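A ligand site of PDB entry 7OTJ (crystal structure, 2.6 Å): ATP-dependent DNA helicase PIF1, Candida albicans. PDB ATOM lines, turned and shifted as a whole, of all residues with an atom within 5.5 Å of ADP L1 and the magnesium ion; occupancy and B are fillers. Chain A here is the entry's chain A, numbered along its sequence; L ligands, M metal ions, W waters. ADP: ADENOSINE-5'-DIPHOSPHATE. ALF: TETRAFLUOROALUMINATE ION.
Asp 107 touches the magnesium ion.
Glu 108 touches the magnesium ion.
The nearest printed residue that does not touch the magnesium ion is Gly 457 (4.3 Å).
Ile 2 touches ADP L1 (CG2 to C6, 3.3 Å).
Ser 26 touches ADP L1.
CB of Phe 190 touches O4' of ADP L1, 3.4 Å away.
Thr 459 touches ADP L1.
Hydrophobic or aromatic side chains that line ADP L1: Ile 2, Val 33 and Phe 190.
The magnesium ion is bound by a fluorine (F1) of ALF L2 (2.0 Å).
The magnesium ion is bound by water W1 (2.0 Å).
The magnesium ion is bound by water W5, at 2.0 Å.
O2B of ADP L1 binds the magnesium ion.
Water W2 is bound to the magnesium ion (2.1 Å).
The magnesium ion is bound by the side-chain hydroxyl (OG) of Ser 32 (2.4 Å).
The magnesium ion has six donor atoms within binding distance.
AL of ALF L2 is bound by O3B of ADP L1.
The backbone NH of Ser 32 sits at hydrogen-bond distance from an oxygen (O1A) of ADP L1, 3.2 Å away.
A nitrogen (N6) of ADP L1 is in hydrogen-bond range of the side-chain amide oxygen (OE1) of Gln 8, 2.8 Å away.
O3B of ADP L1 sits close to N of Gly 28, at 2.8 Å.
The backbone NH (N) of Val 33 lies within hydrogen-bond range of an oxygen (O1A) of ADP L1 (2.9 Å).
An oxygen (O1B) of ADP L1 lies within hydrogen-bond range of the backbone NH (N) of Lys 31, 3.0 Å away.
O1B of ADP L1 is in salt-bridge range of NZ of Lys 31 (3.0 Å).
An oxygen (O3A) of ADP L1 is in hydrogen-bond range of the backbone NH (N) of Gly 30 (3.0 Å).
A nitrogen (N6) of ADP L1 sits at hydrogen-bond distance from the backbone carbonyl oxygen (O) of Ile 3, 3.0 Å away.
An oxygen (O2A) of ADP L1 lies within salt-bridge range of the guanidinium group (NH2) of Arg 191, at 3.2 Å.
N of Thr 29 sits at hydrogen-bond distance from O1B of ADP L1, at 3.2 Å.
OG1 of Thr 29 sits at hydrogen-bond distance from O1B of ADP L1, at 3.3 Å.
A fluorine (F2) of ALF L2 sits at hydrogen-bond distance from the backbone NH (N) of Gly 28, 2.9 Å away.
NZ of Lys 31 sits at hydrogen-bond distance from F3 of ALF L2, 3.0 Å away.
NH1 of Arg 191 is in hydrogen-bond range of F2 of ALF L2.
The backbone NH of Gly 457 sits close to a fluorine (F4) of ALF L2, at 3.5 Å.
The guanidinium group (NH1) of Arg 482 is in hydrogen-bond range of a fluorine (F4) of ALF L2 (2.6 Å).
The side-chain hydroxyl (OG) of Ser 32 sits close to the side-chain carboxylate (OD2) of Asp 107 (2.7 Å).
The backbone carbonyl oxygen (O) of Gly 30 is in hydrogen-bond range of the side-chain amide nitrogen (NE2) of Gln 8 (2.9 Å).
The side-chain amide oxygen (OE1) of Gln 8 lies within hydrogen-bond range of the backbone NH (N) of Ser 5, at 3.0 Å.
The backbone NH of Arg 191 is in hydrogen-bond range of the backbone carbonyl oxygen of Gly 28 (3.3 Å).
The backbone carbonyl oxygen (O) of Gly 28 is in hydrogen-bond range of the backbone NH (N) of Phe 190, at 2.9 Å.
O of Gly 25 is in hydrogen-bond range of NZ of Lys 31, 2.7 Å away.
NE of Arg 191 is in hydrogen-bond range of OG1 of Thr 459, at 2.8 Å.
O of Ser 26 lies within hydrogen-bond range of OG1 of Thr 29 (2.6 Å).
Water W2 lies within hydrogen-bond range of an oxygen (O2A) of ADP L1, the backbone carbonyl oxygen (O) of Gly 457 and the side-chain amide oxygen (OD1) of Asn 62.
Water W4 lies within hydrogen-bond range of O2A of ADP L1 (2.7 Å), OG1 of Thr 459 (2.8 Å) and O of Gly 457 (3.0 Å).
Water W3 lies within hydrogen-bond range of NH2 of Arg 36 (2.9 Å), O1A of ADP L1 (3.1 Å) and OD1 of Asn 62 (3.5 Å).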
ATOM      1  N   ILE A   2       3.327   6.429  26.954  1.00  0.00           N
ATOM      2  CA  ILE A   2       1.935   5.978  26.883  1.00  0.00           C
ATOM      3  C   ILE A   2       1.929   4.538  26.387  1.00  0.00           C
ATOM      4  O   ILE A   2       2.572   4.215  25.384  1.00  0.00           O
ATOM      5  CB  ILE A   2       1.105   6.885  25.959  1.00  0.00           C
ATOM      6  CG1 ILE A   2       0.704   8.196  26.654  1.00  0.00           C
ATOM      7  CG2 ILE A   2      -0.132   6.169  25.451  1.00  0.00           C
ATOM      8  CD1 ILE A   2      -0.064   9.144  25.741  1.00  0.00           C
ATOM      9  N   ILE A   3       1.226   3.664  27.113  1.00  0.00           N
ATOM     10  CA  ILE A   3       0.932   2.317  26.624  1.00  0.00           C
ATOM     11  C   ILE A   3      -0.307   2.371  25.736  1.00  0.00           C
ATOM     12  O   ILE A   3      -1.351   2.914  26.140  1.00  0.00           O
ATOM     13  CB  ILE A   3       0.719   1.351  27.808  1.00  0.00           C
ATOM     14  CG1 ILE A   3       2.005   1.235  28.631  1.00  0.00           C
ATOM     15  CG2 ILE A   3       0.252  -0.006  27.306  1.00  0.00           C
ATOM     16  CD1 ILE A   3       3.220   0.800  27.842  1.00  0.00           C
ATOM     17  N   LEU A   4      -0.209   1.801  24.548  1.00  0.00           N
ATOM     18  CA  LEU A   4      -1.366   1.767  23.653  1.00  0.00           C
ATOM     19  C   LEU A   4      -2.405   0.772  24.154  1.00  0.00           C
ATOM     20  O   LEU A   4      -2.070  -0.333  24.589  1.00  0.00           O
ATOM     21  CB  LEU A   4      -0.931   1.417  22.228  1.00  0.00           C
ATOM     22  CG  LEU A   4      -0.128   2.507  21.501  1.00  0.00           C
ATOM     23  CD1 LEU A   4       0.233   2.066  20.087  1.00  0.00           C
ATOM     24  CD2 LEU A   4      -0.900   3.810  21.477  1.00  0.00           C
ATOM     25  N   SER A   5      -3.669   1.188  24.135  1.00  0.00           N
ATOM     26  CA  SER A   5      -4.760   0.271  24.446  1.00  0.00           C
ATOM     27  C   SER A   5      -4.832  -0.849  23.410  1.00  0.00           C
ATOM     28  O   SER A   5      -4.208  -0.805  22.356  1.00  0.00           O
ATOM     29  CB  SER A   5      -6.085   1.023  24.473  1.00  0.00           C
ATOM     30  OG  SER A   5      -6.409   1.494  23.174  1.00  0.00           O
ATOM     31  N   GLN A   8      -6.161   0.673  20.312  1.00  0.00           N
ATOM     32  CA  GLN A   8      -5.109   1.383  19.590  1.00  0.00           C
ATOM     33  C   GLN A   8      -4.149   0.402  18.927  1.00  0.00           C
ATOM     34  O   GLN A   8      -3.727   0.624  17.787  1.00  0.00           O
ATOM     35  CB  GLN A   8      -4.361   2.324  20.518  1.00  0.00           C
ATOM     36  CG  GLN A   8      -5.138   3.582  20.891  1.00  0.00           C
ATOM     37  CD  GLN A   8      -4.433   4.421  21.950  1.00  0.00           C
ATOM     38  OE1 GLN A   8      -3.885   3.882  22.916  1.00  0.00           O
ATOM     39  NE2 GLN A   8      -4.435   5.724  21.776  1.00  0.00           N
ATOM     40  N   GLY A  25     -13.230   8.201  16.118  1.00  0.00           N
ATOM     41  CA  GLY A  25     -13.541   8.177  17.536  1.00  0.00           C
ATOM     42  C   GLY A  25     -13.712   9.583  18.043  1.00  0.00           C
ATOM     43  O   GLY A  25     -13.272  10.565  17.429  1.00  0.00           O
ATOM     44  N   SER A  26     -14.333   9.700  19.214  1.00  0.00           N
ATOM     45  CA  SER A  26     -14.662  11.001  19.776  1.00  0.00           C
ATOM     46  C   SER A  26     -13.378  11.782  20.085  1.00  0.00           C
ATOM     47  O   SER A  26     -12.268  11.274  20.001  1.00  0.00           O
ATOM     48  CB  SER A  26     -15.480  10.866  21.074  1.00  0.00           C
ATOM     49  OG  SER A  26     -16.746  10.282  20.863  1.00  0.00           O
ATOM     50  N   ALA A  27     -13.561  13.057  20.438  1.00  0.00           N
ATOM     51  CA  ALA A  27     -12.432  13.904  20.796  1.00  0.00           C
ATOM     52  C   ALA A  27     -11.650  13.296  21.956  1.00  0.00           C
ATOM     53  O   ALA A  27     -12.228  12.862  22.957  1.00  0.00           O
ATOM     54  CB  ALA A  27     -12.936  15.301  21.173  1.00  0.00           C
ATOM     55  N   GLY A  28     -10.324  13.267  21.823  1.00  0.00           N
ATOM     56  CA  GLY A  28      -9.489  12.810  22.912  1.00  0.00           C
ATOM     57  C   GLY A  28      -9.391  11.304  23.075  1.00  0.00           C
ATOM     58  O   GLY A  28      -8.990  10.829  24.143  1.00  0.00           O
ATOM     59  N   THR A  29      -9.774  10.542  22.048  1.00  0.00           N
ATOM     60  CA  THR A  29      -9.721   9.092  22.112  1.00  0.00           C
ATOM     61  C   THR A  29      -8.320   8.532  21.815  1.00  0.00           C
ATOM     62  O   THR A  29      -8.168   7.316  21.699  1.00  0.00           O
ATOM     63  CB  THR A  29     -10.733   8.496  21.134  1.00  0.00           C
ATOM     64  OG1 THR A  29     -10.690   9.228  19.895  1.00  0.00           O
ATOM     65  CG2 THR A  29     -12.136   8.589  21.714  1.00  0.00           C
ATOM     66  N   GLY A  30      -7.297   9.383  21.759  1.00  0.00           N
ATOM     67  CA  GLY A  30      -5.952   8.907  21.500  1.00  0.00           C
ATOM     68  C   GLY A  30      -5.660   8.617  20.042  1.00  0.00           C
ATOM     69  O   GLY A  30      -4.808   7.778  19.755  1.00  0.00           O
ATOM     70  N   LYS A  31      -6.350   9.285  19.120  1.00  0.00           N
ATOM     71  CA  LYS A  31      -6.137   9.026  17.703  1.00  0.00           C
ATOM     72  C   LYS A  31      -4.756   9.504  17.261  1.00  0.00           C
ATOM     73  O   LYS A  31      -4.006   8.762  16.629  1.00  0.00           O
ATOM     74  CB  LYS A  31      -7.241   9.686  16.869  1.00  0.00           C
ATOM     75  CG  LYS A  31      -8.608   9.022  17.006  1.00  0.00           C
ATOM     76  CD  LYS A  31      -9.643   9.650  16.048  1.00  0.00           C
ATOM     77  CE  LYS A  31      -9.896  11.124  16.332  1.00  0.00           C
ATOM     78  NZ  LYS A  31     -10.729  11.389  17.542  1.00  0.00           N
ATOM     79  N   SER A  32      -4.387  10.745  17.618  1.00  0.00           N
ATOM     80  CA  SER A  32      -3.092  11.269  17.183  1.00  0.00           C
ATOM     81  C   SER A  32      -1.944  10.603  17.917  1.00  0.00           C
ATOM     82  O   SER A  32      -0.872  10.413  17.354  1.00  0.00           O
ATOM     83  CB  SER A  32      -3.046  12.777  17.364  1.00  0.00           C
ATOM     84  OG  SER A  32      -4.013  13.423  16.573  1.00  0.00           O
ATOM     85  N   VAL A  33      -2.144  10.271  19.197  1.00  0.00           N
ATOM     86  CA  VAL A  33      -1.104   9.539  19.929  1.00  0.00           C
ATOM     87  C   VAL A  33      -0.813   8.220  19.245  1.00  0.00           C
ATOM     88  O   VAL A  33       0.352   7.836  19.057  1.00  0.00           O
ATOM     89  CB  VAL A  33      -1.540   9.343  21.396  1.00  0.00           C
ATOM     90  CG1 VAL A  33      -0.603   8.392  22.100  1.00  0.00           C
ATOM     91  CG2 VAL A  33      -1.572  10.678  22.093  1.00  0.00           C
ATOM     92  N   LEU A  34      -1.866   7.497  18.855  1.00  0.00           N
ATOM     93  CA  LEU A  34      -1.680   6.273  18.064  1.00  0.00           C
ATOM     94  C   LEU A  34      -1.020   6.590  16.727  1.00  0.00           C
ATOM     95  O   LEU A  34      -0.112   5.874  16.290  1.00  0.00           O
ATOM     96  CB  LEU A  34      -3.027   5.599  17.859  1.00  0.00           C
ATOM     97  CG  LEU A  34      -3.096   4.521  16.775  1.00  0.00           C
ATOM     98  CD1 LEU A  34      -2.127   3.372  17.070  1.00  0.00           C
ATOM     99  CD2 LEU A  34      -4.522   4.027  16.661  1.00  0.00           C
ATOM    100  N   ARG A  36       1.120   8.838  15.929  1.00  0.00           N
ATOM    101  CA  ARG A  36       2.573   8.991  16.051  1.00  0.00           C
ATOM    102  C   ARG A  36       3.261   7.648  16.167  1.00  0.00           C
ATOM    103  O   ARG A  36       4.390   7.485  15.677  1.00  0.00           O
ATOM    104  CB  ARG A  36       2.913   9.851  17.264  1.00  0.00           C
ATOM    105  CG  ARG A  36       2.369  11.257  17.218  1.00  0.00           C
ATOM    106  CD  ARG A  36       2.997  12.090  18.314  1.00  0.00           C
ATOM    107  NE  ARG A  36       2.273  13.331  18.540  1.00  0.00           N
ATOM    108  CZ  ARG A  36       1.284  13.463  19.409  1.00  0.00           C
ATOM    109  NH1 ARG A  36       0.879  12.446  20.158  1.00  0.00           N
ATOM    110  NH2 ARG A  36       0.696  14.649  19.551  1.00  0.00           N
ATOM    111  N   ASN A  62       1.238  18.779  15.394  1.00  0.00           N
ATOM    112  CA  ASN A  62       0.916  17.883  16.497  1.00  0.00           C
ATOM    113  C   ASN A  62       1.331  16.439  16.216  1.00  0.00           C
ATOM    114  O   ASN A  62       1.407  15.635  17.145  1.00  0.00           O
ATOM    115  CB  ASN A  62      -0.579  17.965  16.798  1.00  0.00           C
ATOM    116  CG  ASN A  62      -0.976  17.164  18.014  1.00  0.00           C
ATOM    117  OD1 ASN A  62      -1.788  16.252  17.929  1.00  0.00           O
ATOM    118  ND2 ASN A  62      -0.382  17.490  19.158  1.00  0.00           N
ATOM    119  N   ASP A 107      -4.351  13.394   9.187  1.00  0.00           N
ATOM    120  CA  ASP A 107      -5.033  13.610  10.455  1.00  0.00           C
ATOM    121  C   ASP A 107      -6.033  14.758  10.291  1.00  0.00           C
ATOM    122  O   ASP A 107      -5.941  15.567   9.364  1.00  0.00           O
ATOM    123  CB  ASP A 107      -4.032  13.908  11.582  1.00  0.00           C
ATOM    124  CG  ASP A 107      -4.580  13.582  12.977  1.00  0.00           C
ATOM    125  OD1 ASP A 107      -5.809  13.361  13.124  1.00  0.00           O
ATOM    126  OD2 ASP A 107      -3.787  13.539  13.935  1.00  0.00           O
ATOM    127  N   GLU A 108      -7.010  14.793  11.198  1.00  0.00           N
ATOM    128  CA  GLU A 108      -8.093  15.762  11.158  1.00  0.00           C
ATOM    129  C   GLU A 108      -8.766  15.784   9.784  1.00  0.00           C
ATOM    130  O   GLU A 108      -8.891  16.817   9.126  1.00  0.00           O
ATOM    131  CB  GLU A 108      -7.591  17.152  11.557  1.00  0.00           C
ATOM    132  CG  GLU A 108      -7.063  17.237  12.984  1.00  0.00           C
ATOM    133  CD  GLU A 108      -8.145  17.022  14.040  1.00  0.00           C
ATOM    134  OE1 GLU A 108      -7.795  17.000  15.244  1.00  0.00           O
ATOM    135  OE2 GLU A 108      -9.339  16.872  13.690  1.00  0.00           O
ATOM    136  N   PHE A 190      -9.590   9.456  26.614  1.00  0.00           N
ATOM    137  CA  PHE A 190      -8.476   9.677  27.529  1.00  0.00           C
ATOM    138  C   PHE A 190      -8.375  11.111  28.041  1.00  0.00           C
ATOM    139  O   PHE A 190      -8.003  11.319  29.195  1.00  0.00           O
ATOM    140  CB  PHE A 190      -7.156   9.294  26.851  1.00  0.00           C
ATOM    141  CG  PHE A 190      -7.006   7.819  26.573  1.00  0.00           C
ATOM    142  CD1 PHE A 190      -6.732   6.932  27.602  1.00  0.00           C
ATOM    143  CD2 PHE A 190      -7.120   7.329  25.283  1.00  0.00           C
ATOM    144  CE1 PHE A 190      -6.601   5.577  27.352  1.00  0.00           C
ATOM    145  CE2 PHE A 190      -6.983   5.980  25.028  1.00  0.00           C
ATOM    146  CZ  PHE A 190      -6.719   5.103  26.057  1.00  0.00           C
ATOM    147  N   ARG A 191      -8.671  12.105  27.196  1.00  0.00           N
ATOM    148  CA  ARG A 191      -8.414  13.494  27.556  1.00  0.00           C
ATOM    149  C   ARG A 191      -9.173  13.902  28.824  1.00  0.00           C
ATOM    150  O   ARG A 191      -8.629  14.614  29.676  1.00  0.00           O
ATOM    151  CB  ARG A 191      -8.755  14.424  26.402  1.00  0.00           C
ATOM    152  CG  ARG A 191      -8.472  15.888  26.702  1.00  0.00           C
ATOM    153  CD  ARG A 191      -8.725  16.785  25.496  1.00  0.00           C
ATOM    154  NE  ARG A 191      -7.844  16.487  24.375  1.00  0.00           N
ATOM    155  CZ  ARG A 191      -8.260  16.265  23.139  1.00  0.00           C
ATOM    156  NH1 ARG A 191      -9.546  16.283  22.825  1.00  0.00           N
ATOM    157  NH2 ARG A 191      -7.364  16.022  22.184  1.00  0.00           N
ATOM    158  N   GLY A 457      -7.490  19.409  17.602  1.00  0.00           N
ATOM    159  CA  GLY A 457      -6.330  18.546  17.743  1.00  0.00           C
ATOM    160  C   GLY A 457      -5.511  18.805  18.981  1.00  0.00           C
ATOM    161  O   GLY A 457      -4.734  17.943  19.402  1.00  0.00           O
ATOM    162  N   THR A 459      -4.715  19.651  23.051  1.00  0.00           N
ATOM    163  CA  THR A 459      -5.169  19.378  24.409  1.00  0.00           C
ATOM    164  C   THR A 459      -4.773  20.557  25.277  1.00  0.00           C
ATOM    165  O   THR A 459      -3.606  20.986  25.262  1.00  0.00           O
ATOM    166  CB  THR A 459      -4.563  18.082  24.941  1.00  0.00           C
ATOM    167  OG1 THR A 459      -5.080  16.963  24.207  1.00  0.00           O
ATOM    168  CG2 THR A 459      -4.882  17.913  26.413  1.00  0.00           C
ATOM    169  N   ARG A 482     -11.631  20.487  23.984  1.00  0.00           N
ATOM    170  CA  ARG A 482     -10.202  20.727  24.170  1.00  0.00           C
ATOM    171  C   ARG A 482      -9.778  20.591  25.633  1.00  0.00           C
ATOM    172  O   ARG A 482      -8.597  20.341  25.899  1.00  0.00           O
ATOM    173  CB  ARG A 482      -9.818  22.129  23.682  1.00  0.00           C
ATOM    174  CG  ARG A 482     -10.156  22.419  22.221  1.00  0.00           C
ATOM    175  CD  ARG A 482      -9.561  21.397  21.292  1.00  0.00           C
ATOM    176  NE  ARG A 482     -10.484  20.307  21.001  1.00  0.00           N
ATOM    177  CZ  ARG A 482     -10.094  19.135  20.506  1.00  0.00           C
ATOM    178  NH1 ARG A 482      -8.827  18.870  20.272  1.00  0.00           N
ATOM    179  NH2 ARG A 482     -11.018  18.211  20.245  1.00  0.00           N
HETATM  180  PB  ADP L   1      -7.424  12.617  19.637  1.00  0.00           P
HETATM  181  O1B ADP L   1      -8.375  11.469  19.337  1.00  0.00           O
HETATM  182  O2B ADP L   1      -6.375  12.878  18.576  1.00  0.00           O
HETATM  183  O3B ADP L   1      -8.098  13.857  20.154  1.00  0.00           O
HETATM  184  PA  ADP L   1      -5.112  12.675  21.297  1.00  0.00           P
HETATM  185  O1A ADP L   1      -4.118  11.776  20.616  1.00  0.00           O
HETATM  186  O2A ADP L   1      -5.018  14.170  21.148  1.00  0.00           O
HETATM  187  O3A ADP L   1      -6.586  12.133  20.916  1.00  0.00           O
HETATM  188  O5' ADP L   1      -5.112  12.352  22.875  1.00  0.00           O
HETATM  189  C5' ADP L   1      -5.584  13.325  23.801  1.00  0.00           C
HETATM  190  C4' ADP L   1      -4.948  13.050  25.149  1.00  0.00           C
HETATM  191  O4' ADP L   1      -5.145  11.681  25.504  1.00  0.00           O
HETATM  192  C3' ADP L   1      -3.447  13.290  25.081  1.00  0.00           C
HETATM  193  O3' ADP L   1      -3.083  14.222  26.095  1.00  0.00           O
HETATM  194  C2' ADP L   1      -2.799  11.947  25.385  1.00  0.00           C
HETATM  195  O2' ADP L   1      -1.713  12.111  26.292  1.00  0.00           O
HETATM  196  C1' ADP L   1      -3.933  11.127  25.993  1.00  0.00           C
HETATM  197  N9  ADP L   1      -3.836   9.718  25.553  1.00  0.00           N
HETATM  198  C8  ADP L   1      -3.974   9.274  24.294  1.00  0.00           C
HETATM  199  N7  ADP L   1      -3.843   7.929  24.238  1.00  0.00           N
HETATM  200  C5  ADP L   1      -3.607   7.490  25.479  1.00  0.00           C
HETATM  201  C6  ADP L   1      -3.373   6.178  26.126  1.00  0.00           C
HETATM  202  N6  ADP L   1      -3.354   5.028  25.401  1.00  0.00           N
HETATM  203  N1  ADP L   1      -3.168   6.163  27.467  1.00  0.00           N
HETATM  204  C2  ADP L   1      -3.183   7.297  28.197  1.00  0.00           C
HETATM  205  N3  ADP L   1      -3.390   8.517  27.683  1.00  0.00           N
HETATM  206  C4  ADP L   1      -3.602   8.673  26.351  1.00  0.00           C
HETATM  207 AL   ALF L   2      -8.942  15.423  18.813  1.00  0.00          AL
HETATM  208  F1  ALF L   2      -7.892  15.200  17.392  1.00  0.00           F
HETATM  209  F2  ALF L   2      -9.994  15.653  20.241  1.00  0.00           F
HETATM  210  F3  ALF L   2     -10.060  14.220  18.110  1.00  0.00           F
HETATM  211  F4  ALF L   2      -7.801  16.569  19.560  1.00  0.00           F
HETATM  212 MG    MG M   1      -6.177  14.295  17.041  1.00  0.00          MG
HETATM  213  O   HOH W   1      -5.468  15.895  16.065  1.00  0.00           O
HETATM  214  O   HOH W   2      -4.955  15.166  18.567  1.00  0.00           O
HETATM  215  O   HOH W   3      -1.942  14.011  20.609  1.00  0.00           O
HETATM  216  O   HOH W   4      -3.741  16.437  21.753  1.00  0.00           O
HETATM  217  O   HOH W   5      -7.069  13.202  15.609  1.00  0.00           O
